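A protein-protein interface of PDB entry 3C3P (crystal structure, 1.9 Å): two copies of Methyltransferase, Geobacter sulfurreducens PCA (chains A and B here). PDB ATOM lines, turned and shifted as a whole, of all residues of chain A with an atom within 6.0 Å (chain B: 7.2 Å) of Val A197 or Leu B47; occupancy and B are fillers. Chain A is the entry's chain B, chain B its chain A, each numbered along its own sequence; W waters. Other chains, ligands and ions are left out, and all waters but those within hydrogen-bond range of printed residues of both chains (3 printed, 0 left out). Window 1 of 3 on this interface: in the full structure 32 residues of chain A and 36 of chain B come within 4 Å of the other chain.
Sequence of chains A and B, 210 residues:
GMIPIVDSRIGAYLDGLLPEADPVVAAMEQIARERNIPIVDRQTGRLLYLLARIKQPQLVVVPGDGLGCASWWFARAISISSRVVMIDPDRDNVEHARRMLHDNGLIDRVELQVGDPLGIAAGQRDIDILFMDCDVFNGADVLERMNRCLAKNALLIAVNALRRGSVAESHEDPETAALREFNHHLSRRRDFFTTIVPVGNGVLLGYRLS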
ATOM      1  N   LEU A  47     -18.295  -8.049 -25.444  1.00  0.00           N
ATOM      2  CA  LEU A  47     -17.982  -9.320 -24.799  1.00  0.00           C
ATOM      3  C   LEU A  47     -17.758  -9.092 -23.310  1.00  0.00           C
ATOM      4  O   LEU A  47     -18.230  -9.855 -22.495  1.00  0.00           O
ATOM      5  CB  LEU A  47     -16.761  -9.994 -25.429  1.00  0.00           C
ATOM      6  CG  LEU A  47     -16.300 -11.278 -24.734  1.00  0.00           C
ATOM      7  CD1 LEU A  47     -17.370 -12.372 -24.830  1.00  0.00           C
ATOM      8  CD2 LEU A  47     -14.962 -11.722 -25.343  1.00  0.00           C
ATOM      9  N   LEU A 162      -3.469 -11.824 -28.386  1.00  0.00           N
ATOM     10  CA  LEU A 162      -2.906 -12.418 -29.613  1.00  0.00           C
ATOM     11  C   LEU A 162      -2.189 -11.439 -30.536  1.00  0.00           C
ATOM     12  O   LEU A 162      -1.473 -11.834 -31.465  1.00  0.00           O
ATOM     13  CB  LEU A 162      -4.019 -13.076 -30.435  1.00  0.00           C
ATOM     14  CG  LEU A 162      -4.711 -14.295 -29.827  1.00  0.00           C
ATOM     15  CD1 LEU A 162      -5.891 -14.740 -30.715  1.00  0.00           C
ATOM     16  CD2 LEU A 162      -3.677 -15.423 -29.614  1.00  0.00           C
ATOM     17  N   PHE A 193      -8.763 -22.679 -15.577  1.00  0.00           N
ATOM     18  CA  PHE A 193      -9.350 -23.227 -16.833  1.00  0.00           C
ATOM     19  C   PHE A 193      -9.267 -22.027 -17.788  1.00  0.00           C
ATOM     20  O   PHE A 193      -9.972 -21.003 -17.604  1.00  0.00           O
ATOM     21  CB  PHE A 193     -10.772 -23.754 -16.704  1.00  0.00           C
ATOM     22  CG  PHE A 193     -11.295 -24.312 -17.989  1.00  0.00           C
ATOM     23  CD1 PHE A 193     -11.108 -25.654 -18.304  1.00  0.00           C
ATOM     24  CD2 PHE A 193     -11.906 -23.483 -18.923  1.00  0.00           C
ATOM     25  CE1 PHE A 193     -11.589 -26.142 -19.518  1.00  0.00           C
ATOM     26  CE2 PHE A 193     -12.359 -23.970 -20.126  1.00  0.00           C
ATOM     27  CZ  PHE A 193     -12.200 -25.301 -20.418  1.00  0.00           C
ATOM     28  N   THR A 195      -9.057 -20.182 -21.783  1.00  0.00           N
ATOM     29  CA  THR A 195      -9.277 -20.255 -23.242  1.00  0.00           C
ATOM     30  C   THR A 195      -9.053 -18.860 -23.804  1.00  0.00           C
ATOM     31  O   THR A 195      -9.218 -17.859 -23.097  1.00  0.00           O
ATOM     32  CB  THR A 195     -10.644 -20.841 -23.636  1.00  0.00           C
ATOM     33  OG1 THR A 195     -10.607 -21.222 -25.027  1.00  0.00           O
ATOM     34  CG2 THR A 195     -11.748 -19.821 -23.376  1.00  0.00           C
ATOM     35  N   ILE A 196      -8.583 -18.802 -25.037  1.00  0.00           N
ATOM     36  CA  ILE A 196      -8.349 -17.527 -25.703  1.00  0.00           C
ATOM     37  C   ILE A 196      -9.317 -17.442 -26.875  1.00  0.00           C
ATOM     38  O   ILE A 196      -9.278 -18.251 -27.827  1.00  0.00           O
ATOM     39  CB  ILE A 196      -6.900 -17.315 -26.179  1.00  0.00           C
ATOM     40  CG1 ILE A 196      -5.931 -17.421 -25.008  1.00  0.00           C
ATOM     41  CG2 ILE A 196      -6.790 -15.955 -26.888  1.00  0.00           C
ATOM     42  CD1 ILE A 196      -4.470 -17.266 -25.415  1.00  0.00           C
ATOM     43  N   VAL A 197     -10.229 -16.495 -26.755  1.00  0.00           N
ATOM     44  CA  VAL A 197     -11.221 -16.315 -27.816  1.00  0.00           C
ATOM     45  C   VAL A 197     -10.751 -15.265 -28.837  1.00  0.00           C
ATOM     46  O   VAL A 197     -10.192 -14.209 -28.510  1.00  0.00           O
ATOM     47  CB  VAL A 197     -12.649 -16.057 -27.313  1.00  0.00           C
ATOM     48  CG1 VAL A 197     -13.161 -17.292 -26.514  1.00  0.00           C
ATOM     49  CG2 VAL A 197     -12.747 -14.753 -26.523  1.00  0.00           C
ATOM     50  N   PRO A 198     -10.966 -15.592 -30.116  1.00  0.00           N
ATOM     51  CA  PRO A 198     -10.499 -14.713 -31.146  1.00  0.00           C
ATOM     52  C   PRO A 198     -11.448 -13.582 -31.442  1.00  0.00           C
ATOM     53  O   PRO A 198     -12.028 -13.514 -32.503  1.00  0.00           O
ATOM     54  CB  PRO A 198     -10.312 -15.646 -32.353  1.00  0.00           C
ATOM     55  CG  PRO A 198     -11.249 -16.737 -32.151  1.00  0.00           C
ATOM     56  CD  PRO A 198     -11.610 -16.797 -30.670  1.00  0.00           C
ATOM     57  N   VAL A 199     -11.535 -12.715 -30.445  1.00  0.00           N
ATOM     58  CA  VAL A 199     -12.350 -11.483 -30.527  1.00  0.00           C
ATOM     59  C   VAL A 199     -11.381 -10.303 -30.482  1.00  0.00           C
ATOM     60  O   VAL A 199     -10.410 -10.274 -29.745  1.00  0.00           O
ATOM     61  CB  VAL A 199     -13.466 -11.387 -29.455  1.00  0.00           C
ATOM     62  CG1 VAL A 199     -12.895 -11.458 -28.072  1.00  0.00           C
ATOM     63  CG2 VAL A 199     -14.283 -10.098 -29.637  1.00  0.00           C
ATOM     64  N   GLY A 200     -11.636  -9.340 -31.353  1.00  0.00           N
ATOM     65  CA  GLY A 200     -10.765  -8.157 -31.447  1.00  0.00           C
ATOM     66  C   GLY A 200      -9.328  -8.622 -31.580  1.00  0.00           C
ATOM     67  O   GLY A 200      -9.001  -9.380 -32.471  1.00  0.00           O
ATOM     68  N   ASN A 201      -8.451  -8.199 -30.681  1.00  0.00           N
ATOM     69  CA  ASN A 201      -7.030  -8.637 -30.733  1.00  0.00           C
ATOM     70  C   ASN A 201      -6.695  -9.849 -29.879  1.00  0.00           C
ATOM     71  O   ASN A 201      -5.539 -10.085 -29.529  1.00  0.00           O
ATOM     72  CB  ASN A 201      -6.078  -7.476 -30.509  1.00  0.00           C
ATOM     73  CG  ASN A 201      -5.886  -6.680 -31.794  1.00  0.00           C
ATOM     74  OD1 ASN A 201      -5.411  -7.224 -32.806  1.00  0.00           O
ATOM     75  ND2 ASN A 201      -6.207  -5.409 -31.757  1.00  0.00           N
ATOM     76  N   GLY A 202      -7.740 -10.631 -29.601  1.00  0.00           N
ATOM     77  CA  GLY A 202      -7.606 -11.855 -28.825  1.00  0.00           C
ATOM     78  C   GLY A 202      -7.858 -11.542 -27.371  1.00  0.00           C
ATOM     79  O   GLY A 202      -7.286 -10.588 -26.840  1.00  0.00           O
ATOM     80  N   VAL A 203      -8.717 -12.339 -26.754  1.00  0.00           N
ATOM     81  CA  VAL A 203      -9.087 -12.176 -25.341  1.00  0.00           C
ATOM     82  C   VAL A 203      -8.923 -13.485 -24.599  1.00  0.00           C
ATOM     83  O   VAL A 203      -9.563 -14.506 -24.874  1.00  0.00           O
ATOM     84  CB  VAL A 203     -10.575 -11.638 -25.162  1.00  0.00           C
ATOM     85  CG1 VAL A 203     -10.944 -11.469 -23.661  1.00  0.00           C
ATOM     86  CG2 VAL A 203     -10.814 -10.342 -25.946  1.00  0.00           C
ATOM     87  N   LEU A 204      -7.987 -13.452 -23.683  1.00  0.00           N
ATOM     88  CA  LEU A 204      -7.707 -14.583 -22.838  1.00  0.00           C
ATOM     89  C   LEU A 204      -8.668 -14.524 -21.660  1.00  0.00           C
ATOM     90  O   LEU A 204      -8.842 -13.485 -21.032  1.00  0.00           O
ATOM     91  CB  LEU A 204      -6.260 -14.567 -22.346  1.00  0.00           C
ATOM     92  CG  LEU A 204      -5.918 -15.654 -21.308  1.00  0.00           C
ATOM     93  CD1 LEU A 204      -4.462 -16.075 -21.397  1.00  0.00           C
ATOM     94  CD2 LEU A 204      -6.318 -15.279 -19.870  1.00  0.00           C
ATOM     95  N   LEU A 205      -9.319 -15.641 -21.412  1.00  0.00           N
ATOM     96  CA  LEU A 205     -10.231 -15.787 -20.292  1.00  0.00           C
ATOM     97  C   LEU A 205      -9.685 -16.878 -19.393  1.00  0.00           C
ATOM     98  O   LEU A 205      -9.560 -18.043 -19.807  1.00  0.00           O
ATOM     99  CB  LEU A 205     -11.619 -16.189 -20.765  1.00  0.00           C
ATOM    100  CG  LEU A 205     -12.221 -15.255 -21.766  1.00  0.00           C
ATOM    101  CD1 LEU A 205     -13.477 -15.888 -22.366  1.00  0.00           C
ATOM    102  CD2 LEU A 205     -12.508 -13.871 -21.071  1.00  0.00           C
ATOM    103  N   VAL B   6     -11.130 -18.310 -38.258  1.00  0.00           N
ATOM    104  CA  VAL B   6      -9.846 -17.973 -37.618  1.00  0.00           C
ATOM    105  C   VAL B   6      -8.665 -18.323 -38.559  1.00  0.00           C
ATOM    106  O   VAL B   6      -8.671 -19.366 -39.212  1.00  0.00           O
ATOM    107  CB  VAL B   6      -9.672 -18.689 -36.226  1.00  0.00           C
ATOM    108  CG1 VAL B   6      -8.371 -18.262 -35.550  1.00  0.00           C
ATOM    109  CG2 VAL B   6     -10.883 -18.412 -35.278  1.00  0.00           C
ATOM    110  N   LEU B  14      -3.461 -21.559 -31.119  1.00  0.00           N
ATOM    111  CA  LEU B  14      -4.446 -21.774 -30.051  1.00  0.00           C
ATOM    112  C   LEU B  14      -4.552 -23.256 -29.729  1.00  0.00           C
ATOM    113  O   LEU B  14      -4.636 -23.663 -28.578  1.00  0.00           O
ATOM    114  CB  LEU B  14      -5.819 -21.188 -30.429  1.00  0.00           C
ATOM    115  CG  LEU B  14      -5.873 -19.662 -30.569  1.00  0.00           C
ATOM    116  CD1 LEU B  14      -7.231 -19.171 -31.087  1.00  0.00           C
ATOM    117  CD2 LEU B  14      -5.539 -19.019 -29.233  1.00  0.00           C
ATOM    118  N   ASP B  41     -16.224 -28.817 -31.819  1.00  0.00           N
ATOM    119  CA  ASP B  41     -14.744 -28.972 -31.706  1.00  0.00           C
ATOM    120  C   ASP B  41     -14.259 -28.614 -30.277  1.00  0.00           C
ATOM    121  O   ASP B  41     -15.019 -28.074 -29.463  1.00  0.00           O
ATOM    122  CB  ASP B  41     -13.898 -28.289 -32.820  1.00  0.00           C
ATOM    123  CG  ASP B  41     -13.865 -26.754 -32.789  1.00  0.00           C
ATOM    124  OD1 ASP B  41     -14.298 -26.058 -31.838  1.00  0.00           O
ATOM    125  OD2 ASP B  41     -13.288 -26.219 -33.764  1.00  0.00           O
ATOM    126  N   ARG B  42     -12.990 -28.890 -29.997  1.00  0.00           N
ATOM    127  CA  ARG B  42     -12.448 -28.643 -28.631  1.00  0.00           C
ATOM    128  C   ARG B  42     -12.436 -27.204 -28.181  1.00  0.00           C
ATOM    129  O   ARG B  42     -12.743 -26.937 -27.036  1.00  0.00           O
ATOM    130  CB  ARG B  42     -11.038 -29.213 -28.432  1.00  0.00           C
ATOM    131  CG  ARG B  42     -10.979 -30.722 -28.297  1.00  0.00           C
ATOM    132  CD  ARG B  42      -9.531 -31.203 -28.138  1.00  0.00           C
ATOM    133  NE  ARG B  42      -8.882 -30.825 -26.872  1.00  0.00           N
ATOM    134  CZ  ARG B  42      -7.571 -30.983 -26.655  1.00  0.00           C
ATOM    135  NH1 ARG B  42      -6.797 -31.405 -27.632  1.00  0.00           N
ATOM    136  NH2 ARG B  42      -7.012 -30.643 -25.508  1.00  0.00           N
ATOM    137  N   GLN B  43     -12.079 -26.276 -29.057  1.00  0.00           N
ATOM    138  CA  GLN B  43     -12.036 -24.867 -28.662  1.00  0.00           C
ATOM    139  C   GLN B  43     -13.440 -24.413 -28.289  1.00  0.00           C
ATOM    140  O   GLN B  43     -13.637 -23.623 -27.360  1.00  0.00           O
ATOM    141  CB  GLN B  43     -11.486 -23.978 -29.779  1.00  0.00           C
ATOM    142  CG  GLN B  43     -10.025 -24.259 -30.130  1.00  0.00           C
ATOM    143  CD  GLN B  43      -9.073 -23.897 -29.015  1.00  0.00           C
ATOM    144  OE1 GLN B  43      -9.475 -23.323 -28.012  1.00  0.00           O
ATOM    145  NE2 GLN B  43      -7.797 -24.182 -29.212  1.00  0.00           N
ATOM    146  N   THR B  44     -14.423 -24.934 -29.025  1.00  0.00           N
ATOM    147  CA  THR B  44     -15.815 -24.580 -28.802  1.00  0.00           C
ATOM    148  C   THR B  44     -16.335 -25.203 -27.513  1.00  0.00           C
ATOM    149  O   THR B  44     -17.007 -24.541 -26.730  1.00  0.00           O
ATOM    150  CB  THR B  44     -16.714 -24.950 -30.033  1.00  0.00           C
ATOM    151  OG1 THR B  44     -16.227 -24.236 -31.179  1.00  0.00           O
ATOM    152  CG2 THR B  44     -18.168 -24.576 -29.795  1.00  0.00           C
ATOM    153  N   GLY B  45     -16.005 -26.458 -27.284  1.00  0.00           N
ATOM    154  CA  GLY B  45     -16.451 -27.146 -26.079  1.00  0.00           C
ATOM    155  C   GLY B  45     -15.873 -26.459 -24.851  1.00  0.00           C
ATOM    156  O   GLY B  45     -16.554 -26.294 -23.847  1.00  0.00           O
ATOM    157  N   ARG B  46     -14.610 -26.059 -24.948  1.00  0.00           N
ATOM    158  CA  ARG B  46     -13.937 -25.377 -23.814  1.00  0.00           C
ATOM    159  C   ARG B  46     -14.662 -24.063 -23.492  1.00  0.00           C
ATOM    160  O   ARG B  46     -14.841 -23.696 -22.342  1.00  0.00           O
ATOM    161  CB  ARG B  46     -12.436 -25.172 -24.077  1.00  0.00           C
ATOM    162  CG  ARG B  46     -11.640 -26.474 -24.097  1.00  0.00           C
ATOM    163  CD  ARG B  46     -10.138 -26.267 -24.312  1.00  0.00           C
ATOM    164  NE  ARG B  46      -9.497 -25.455 -23.278  1.00  0.00           N
ATOM    165  CZ  ARG B  46      -9.059 -25.948 -22.127  1.00  0.00           C
ATOM    166  NH1 ARG B  46      -9.211 -27.227 -21.854  1.00  0.00           N
ATOM    167  NH2 ARG B  46      -8.495 -25.168 -21.232  1.00  0.00           N
ATOM    168  N   LEU B  47     -15.151 -23.394 -24.524  1.00  0.00           N
ATOM    169  CA  LEU B  47     -15.881 -22.130 -24.325  1.00  0.00           C
ATOM    170  C   LEU B  47     -17.182 -22.437 -23.635  1.00  0.00           C
ATOM    171  O   LEU B  47     -17.594 -21.700 -22.747  1.00  0.00           O
ATOM    172  CB  LEU B  47     -16.163 -21.391 -25.619  1.00  0.00           C
ATOM    173  CG  LEU B  47     -16.934 -20.075 -25.441  1.00  0.00           C
ATOM    174  CD1 LEU B  47     -16.141 -19.074 -24.606  1.00  0.00           C
ATOM    175  CD2 LEU B  47     -17.324 -19.520 -26.821  1.00  0.00           C
ATOM    176  N   LEU B  48     -17.818 -23.534 -24.029  1.00  0.00           N
ATOM    177  CA  LEU B  48     -19.093 -23.939 -23.415  1.00  0.00           C
ATOM    178  C   LEU B  48     -18.896 -24.176 -21.928  1.00  0.00           C
ATOM    179  O   LEU B  48     -19.667 -23.744 -21.087  1.00  0.00           O
ATOM    180  CB  LEU B  48     -19.653 -25.221 -24.023  1.00  0.00           C
ATOM    181  CG  LEU B  48     -20.106 -25.184 -25.497  1.00  0.00           C
ATOM    182  CD1 LEU B  48     -20.779 -26.515 -25.912  1.00  0.00           C
ATOM    183  CD2 LEU B  48     -21.052 -24.062 -25.761  1.00  0.00           C
ATOM    184  N   TYR B  49     -17.861 -24.932 -21.636  1.00  0.00           N
ATOM    185  CA  TYR B  49     -17.495 -25.222 -20.236  1.00  0.00           C
ATOM    186  C   TYR B  49     -17.293 -23.946 -19.421  1.00  0.00           C
ATOM    187  O   TYR B  49     -17.843 -23.793 -18.346  1.00  0.00           O
ATOM    188  CB  TYR B  49     -16.223 -26.074 -20.157  1.00  0.00           C
ATOM    189  CG  TYR B  49     -15.776 -26.366 -18.712  1.00  0.00           C
ATOM    190  CD1 TYR B  49     -16.259 -27.468 -18.011  1.00  0.00           C
ATOM    191  CD2 TYR B  49     -14.895 -25.512 -18.059  1.00  0.00           C
ATOM    192  CE1 TYR B  49     -15.846 -27.726 -16.690  1.00  0.00           C
ATOM    193  CE2 TYR B  49     -14.491 -25.743 -16.748  1.00  0.00           C
ATOM    194  CZ  TYR B  49     -14.975 -26.852 -16.065  1.00  0.00           C
ATOM    195  OH  TYR B  49     -14.553 -27.061 -14.768  1.00  0.00           O
ATOM    196  N   LEU B  50     -16.506 -23.029 -19.965  1.00  0.00           N
ATOM    197  CA  LEU B  50     -16.190 -21.793 -19.261  1.00  0.00           C
ATOM    198  C   LEU B  50     -17.437 -20.954 -19.031  1.00  0.00           C
ATOM    199  O   LEU B  50     -17.660 -20.439 -17.930  1.00  0.00           O
ATOM    200  CB  LEU B  50     -15.058 -21.001 -19.945  1.00  0.00           C
ATOM    201  CG  LEU B  50     -14.576 -19.801 -19.099  1.00  0.00           C
ATOM    202  CD1 LEU B  50     -13.043 -19.587 -19.162  1.00  0.00           C
ATOM    203  CD2 LEU B  50     -15.397 -18.528 -19.476  1.00  0.00           C
ATOM    204  N   LEU B  51     -18.269 -20.832 -20.054  1.00  0.00           N
ATOM    205  CA  LEU B  51     -19.490 -20.019 -19.905  1.00  0.00           C
ATOM    206  C   LEU B  51     -20.419 -20.610 -18.836  1.00  0.00           C
ATOM    207  O   LEU B  51     -21.066 -19.907 -18.037  1.00  0.00           O
ATOM    208  CB  LEU B  51     -20.218 -19.900 -21.267  1.00  0.00           C
ATOM    209  CG  LEU B  51     -19.526 -19.067 -22.351  1.00  0.00           C
ATOM    210  CD1 LEU B  51     -20.245 -19.241 -23.687  1.00  0.00           C
ATOM    211  CD2 LEU B  51     -19.422 -17.590 -21.957  1.00  0.00           C
ATOM    212  N   ALA B  52     -20.463 -21.930 -18.799  1.00  0.00           N
ATOM    213  CA  ALA B  52     -21.328 -22.649 -17.870  1.00  0.00           C
ATOM    214  C   ALA B  52     -20.801 -22.473 -16.462  1.00  0.00           C
ATOM    215  O   ALA B  52     -21.554 -22.255 -15.529  1.00  0.00           O
ATOM    216  CB  ALA B  52     -21.446 -24.145 -18.248  1.00  0.00           C
ATOM    217  N   ARG B  53     -19.487 -22.531 -16.310  1.00  0.00           N
ATOM    218  CA  ARG B  53     -18.907 -22.306 -14.978  1.00  0.00           C
ATOM    219  C   ARG B  53     -19.235 -20.901 -14.451  1.00  0.00           C
ATOM    220  O   ARG B  53     -19.596 -20.728 -13.306  1.00  0.00           O
ATOM    221  CB  ARG B  53     -17.395 -22.477 -14.947  1.00  0.00           C
ATOM    222  CG  ARG B  53     -16.880 -23.895 -15.018  1.00  0.00           C
ATOM    223  CD  ARG B  53     -17.465 -24.831 -13.944  1.00  0.00           C
ATOM    224  NE  ARG B  53     -17.207 -24.457 -12.552  1.00  0.00           N
ATOM    225  CZ  ARG B  53     -16.179 -24.880 -11.821  1.00  0.00           C
ATOM    226  NH1 ARG B  53     -15.237 -25.673 -12.330  1.00  0.00           N
ATOM    227  NH2 ARG B  53     -16.088 -24.459 -10.576  1.00  0.00           N
ATOM    228  N   TRP B  73     -19.722 -31.579 -22.190  1.00  0.00           N
ATOM    229  CA  TRP B  73     -19.037 -30.337 -21.749  1.00  0.00           C
ATOM    230  C   TRP B  73     -19.790 -29.648 -20.628  1.00  0.00           C
ATOM    231  O   TRP B  73     -19.215 -29.216 -19.625  1.00  0.00           O
ATOM    232  CB  TRP B  73     -18.804 -29.353 -22.908  1.00  0.00           C
ATOM    233  CG  TRP B  73     -17.783 -29.843 -23.886  1.00  0.00           C
ATOM    234  CD1 TRP B  73     -18.020 -30.500 -25.063  1.00  0.00           C
ATOM    235  CD2 TRP B  73     -16.368 -29.758 -23.747  1.00  0.00           C
ATOM    236  NE1 TRP B  73     -16.821 -30.812 -25.675  1.00  0.00           N
ATOM    237  CE2 TRP B  73     -15.794 -30.385 -24.878  1.00  0.00           C
ATOM    238  CE3 TRP B  73     -15.519 -29.254 -22.755  1.00  0.00           C
ATOM    239  CZ2 TRP B  73     -14.422 -30.474 -25.067  1.00  0.00           C
ATOM    240  CZ3 TRP B  73     -14.156 -29.353 -22.941  1.00  0.00           C
ATOM    241  CH2 TRP B  73     -13.622 -29.965 -24.091  1.00  0.00           C
ATOM    242  N   PHE B  74     -21.099 -29.577 -20.801  1.00  0.00           N
ATOM    243  CA  PHE B  74     -21.963 -28.948 -19.795  1.00  0.00           C
ATOM    244  C   PHE B  74     -22.041 -29.737 -18.469  1.00  0.00           C
ATOM    245  O   PHE B  74     -22.053 -29.144 -17.376  1.00  0.00           O
ATOM    246  CB  PHE B  74     -23.380 -28.713 -20.332  1.00  0.00           C
ATOM    247  CG  PHE B  74     -23.467 -27.654 -21.394  1.00  0.00           C
ATOM    248  CD1 PHE B  74     -23.100 -26.339 -21.100  1.00  0.00           C
ATOM    249  CD2 PHE B  74     -24.004 -27.928 -22.633  1.00  0.00           C
ATOM    250  CE1 PHE B  74     -23.202 -25.328 -22.052  1.00  0.00           C
ATOM    251  CE2 PHE B  74     -24.118 -26.911 -23.588  1.00  0.00           C
ATOM    252  CZ  PHE B  74     -23.720 -25.615 -23.289  1.00  0.00           C
ATOM    253  N   ILE B 157     -26.975 -20.201 -26.237  1.00  0.00           N
ATOM    254  CA  ILE B 157     -25.684 -20.566 -26.885  1.00  0.00           C
ATOM    255  C   ILE B 157     -26.056 -21.327 -28.165  1.00  0.00           C
ATOM    256  O   ILE B 157     -26.579 -22.454 -28.121  1.00  0.00           O
ATOM    257  CB  ILE B 157     -24.732 -21.402 -26.013  1.00  0.00           C
ATOM    258  CG1 ILE B 157     -24.469 -20.713 -24.664  1.00  0.00           C
ATOM    259  CG2 ILE B 157     -23.418 -21.654 -26.789  1.00  0.00           C
ATOM    260  CD1 ILE B 157     -23.609 -21.516 -23.699  1.00  0.00           C
ATOM    261  N   VAL B 197     -19.029 -14.826 -31.094  1.00  0.00           N
ATOM    262  CA  VAL B 197     -17.595 -15.030 -30.931  1.00  0.00           C
ATOM    263  C   VAL B 197     -17.155 -15.967 -32.073  1.00  0.00           C
ATOM    264  O   VAL B 197     -17.723 -17.027 -32.353  1.00  0.00           O
ATOM    265  CB  VAL B 197     -17.154 -15.471 -29.515  1.00  0.00           C
ATOM    266  CG1 VAL B 197     -17.536 -14.374 -28.478  1.00  0.00           C
ATOM    267  CG2 VAL B 197     -17.722 -16.826 -29.142  1.00  0.00           C
ATOM    268  N   PRO B 198     -16.131 -15.545 -32.773  1.00  0.00           N
ATOM    269  CA  PRO B 198     -15.789 -16.401 -33.892  1.00  0.00           C
ATOM    270  C   PRO B 198     -14.870 -17.593 -33.611  1.00  0.00           C
ATOM    271  O   PRO B 198     -13.817 -17.726 -34.247  1.00  0.00           O
ATOM    272  CB  PRO B 198     -15.156 -15.420 -34.875  1.00  0.00           C
ATOM    273  CG  PRO B 198     -14.608 -14.412 -34.077  1.00  0.00           C
ATOM    274  CD  PRO B 198     -15.446 -14.251 -32.842  1.00  0.00           C
ATOM    275  N   VAL B 199     -15.292 -18.395 -32.635  1.00  0.00           N
ATOM    276  CA  VAL B 199     -14.586 -19.641 -32.256  1.00  0.00           C
ATOM    277  C   VAL B 199     -15.246 -20.768 -33.046  1.00  0.00           C
ATOM    278  O   VAL B 199     -16.445 -20.815 -33.202  1.00  0.00           O
ATOM    279  CB  VAL B 199     -14.627 -19.965 -30.737  1.00  0.00           C
ATOM    280  CG1 VAL B 199     -16.036 -20.170 -30.241  1.00  0.00           C
ATOM    281  CG2 VAL B 199     -13.804 -21.219 -30.441  1.00  0.00           C
ATOM    282  N   VAL B 203     -20.019 -18.850 -32.694  1.00  0.00           N
ATOM    283  CA  VAL B 203     -20.918 -19.094 -31.573  1.00  0.00           C
ATOM    284  C   VAL B 203     -21.699 -17.823 -31.222  1.00  0.00           C
ATOM    285  O   VAL B 203     -21.131 -16.807 -30.860  1.00  0.00           O
ATOM    286  CB  VAL B 203     -20.152 -19.613 -30.307  1.00  0.00           C
ATOM    287  CG1 VAL B 203     -21.153 -19.892 -29.153  1.00  0.00           C
ATOM    288  CG2 VAL B 203     -19.318 -20.884 -30.628  1.00  0.00           C
ATOM    289  N   LEU B 205     -24.118 -15.824 -28.867  1.00  0.00           N
ATOM    290  CA  LEU B 205     -24.460 -15.768 -27.453  1.00  0.00           C
ATOM    291  C   LEU B 205     -25.514 -14.702 -27.249  1.00  0.00           C
ATOM    292  O   LEU B 205     -25.375 -13.556 -27.720  1.00  0.00           O
ATOM    293  CB  LEU B 205     -23.215 -15.438 -26.616  1.00  0.00           C
ATOM    294  CG  LEU B 205     -21.995 -16.357 -26.745  1.00  0.00           C
ATOM    295  CD1 LEU B 205     -20.752 -15.805 -25.980  1.00  0.00           C
ATOM    296  CD2 LEU B 205     -22.358 -17.741 -26.260  1.00  0.00           C
HETATM  297  O   HOH W   1      -9.121 -23.320 -25.352  1.00  0.00           O
HETATM  298  O   HOH W   2     -12.441 -21.105 -26.935  1.00  0.00           O
HETATM  299  O   HOH W   3      -7.905 -20.750 -27.150  1.00  0.00           O
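O of Val A203 sits at hydrogen-bond distance from N of Val A197, 2.8 Å away. OH of Tyr B49 is in hydrogen-bond range of NH1 of Arg B53 (2.9 Å). The backbone carbonyl oxygen (O) of Leu B14 is in hydrogen-bond range of the side-chain amide nitrogen (NE2) of Gln B43. The backbone carbonyl oxygen (O) of Thr A195 is in hydrogen-bond range of the backbone NH (N) of Leu A205, 2.8 Å away.
Arg B46 touches Phe A193. Phe A193 touches Tyr B49. Leu B50 touches Phe A193 (CD1 to O, 3.7 Å). Thr A195 touches Gln B43. Leu B14 touches Ile A196. Val A197 touches Leu B47 (CG1 to CD1, 3.96 Å). Val B6 touches Pro A198 (CG2 to CG, 3.6 Å). Pro B198 touches Pro A198 (CG to O, 3.2 Å). Leu B50 touches Leu A205.
Printed residues of chain B within 4 Å of Phe A193: Arg B46, Tyr B49 and Leu B50. Of the printed residues of chain B, Pro A198 touches Val B6 and Pro B198. Gly A202 touches none of the printed residues of chain B. Of the printed residues of chain A, Leu B47 touches Val A197 (3.96 Å). Leu B51 touches none of the printed residues of chain A.
Of the 14 printed residues of chain A, 6 touch a printed residue of chain B. Hydrophobic or aromatic side chains of chain A within 4 Å of the printed part of chain B: Phe A193, Ile A196, Val A197 and Pro A198. Of the 23 printed residues of chain B, 8 touch a printed residue of chain A. Among the printed residues, no Asp or Glu carboxylate lies within 4 Å of a Lys or Arg side-chain nitrogen of the other chain.
Val A197 touches Leu B47, but with the chains exchanged Leu A47 does not touch Val B197 (4.2 Å). Pro B198 touches its own counterpart, Pro A198. Of the 9 pairs that touch across the chains among the printed residues, 1 has its exchanged pair printed and touching as well.
Water W1 lies within hydrogen-bond range of OG1 of Thr A195 (2.6 Å), OE1 of Gln B43 (2.7 Å) and NE of Arg B46 (3.0 Å). Water W2 lies within hydrogen-bond range of OG1 of Thr A195 (2.6 Å) and O of Gln B43 (2.8 Å). Water W3 lies within hydrogen-bond range of the backbone carbonyl oxygen of Ile A196, the side-chain amide oxygen of Gln B43 and the side-chain hydroxyl of Thr A195.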
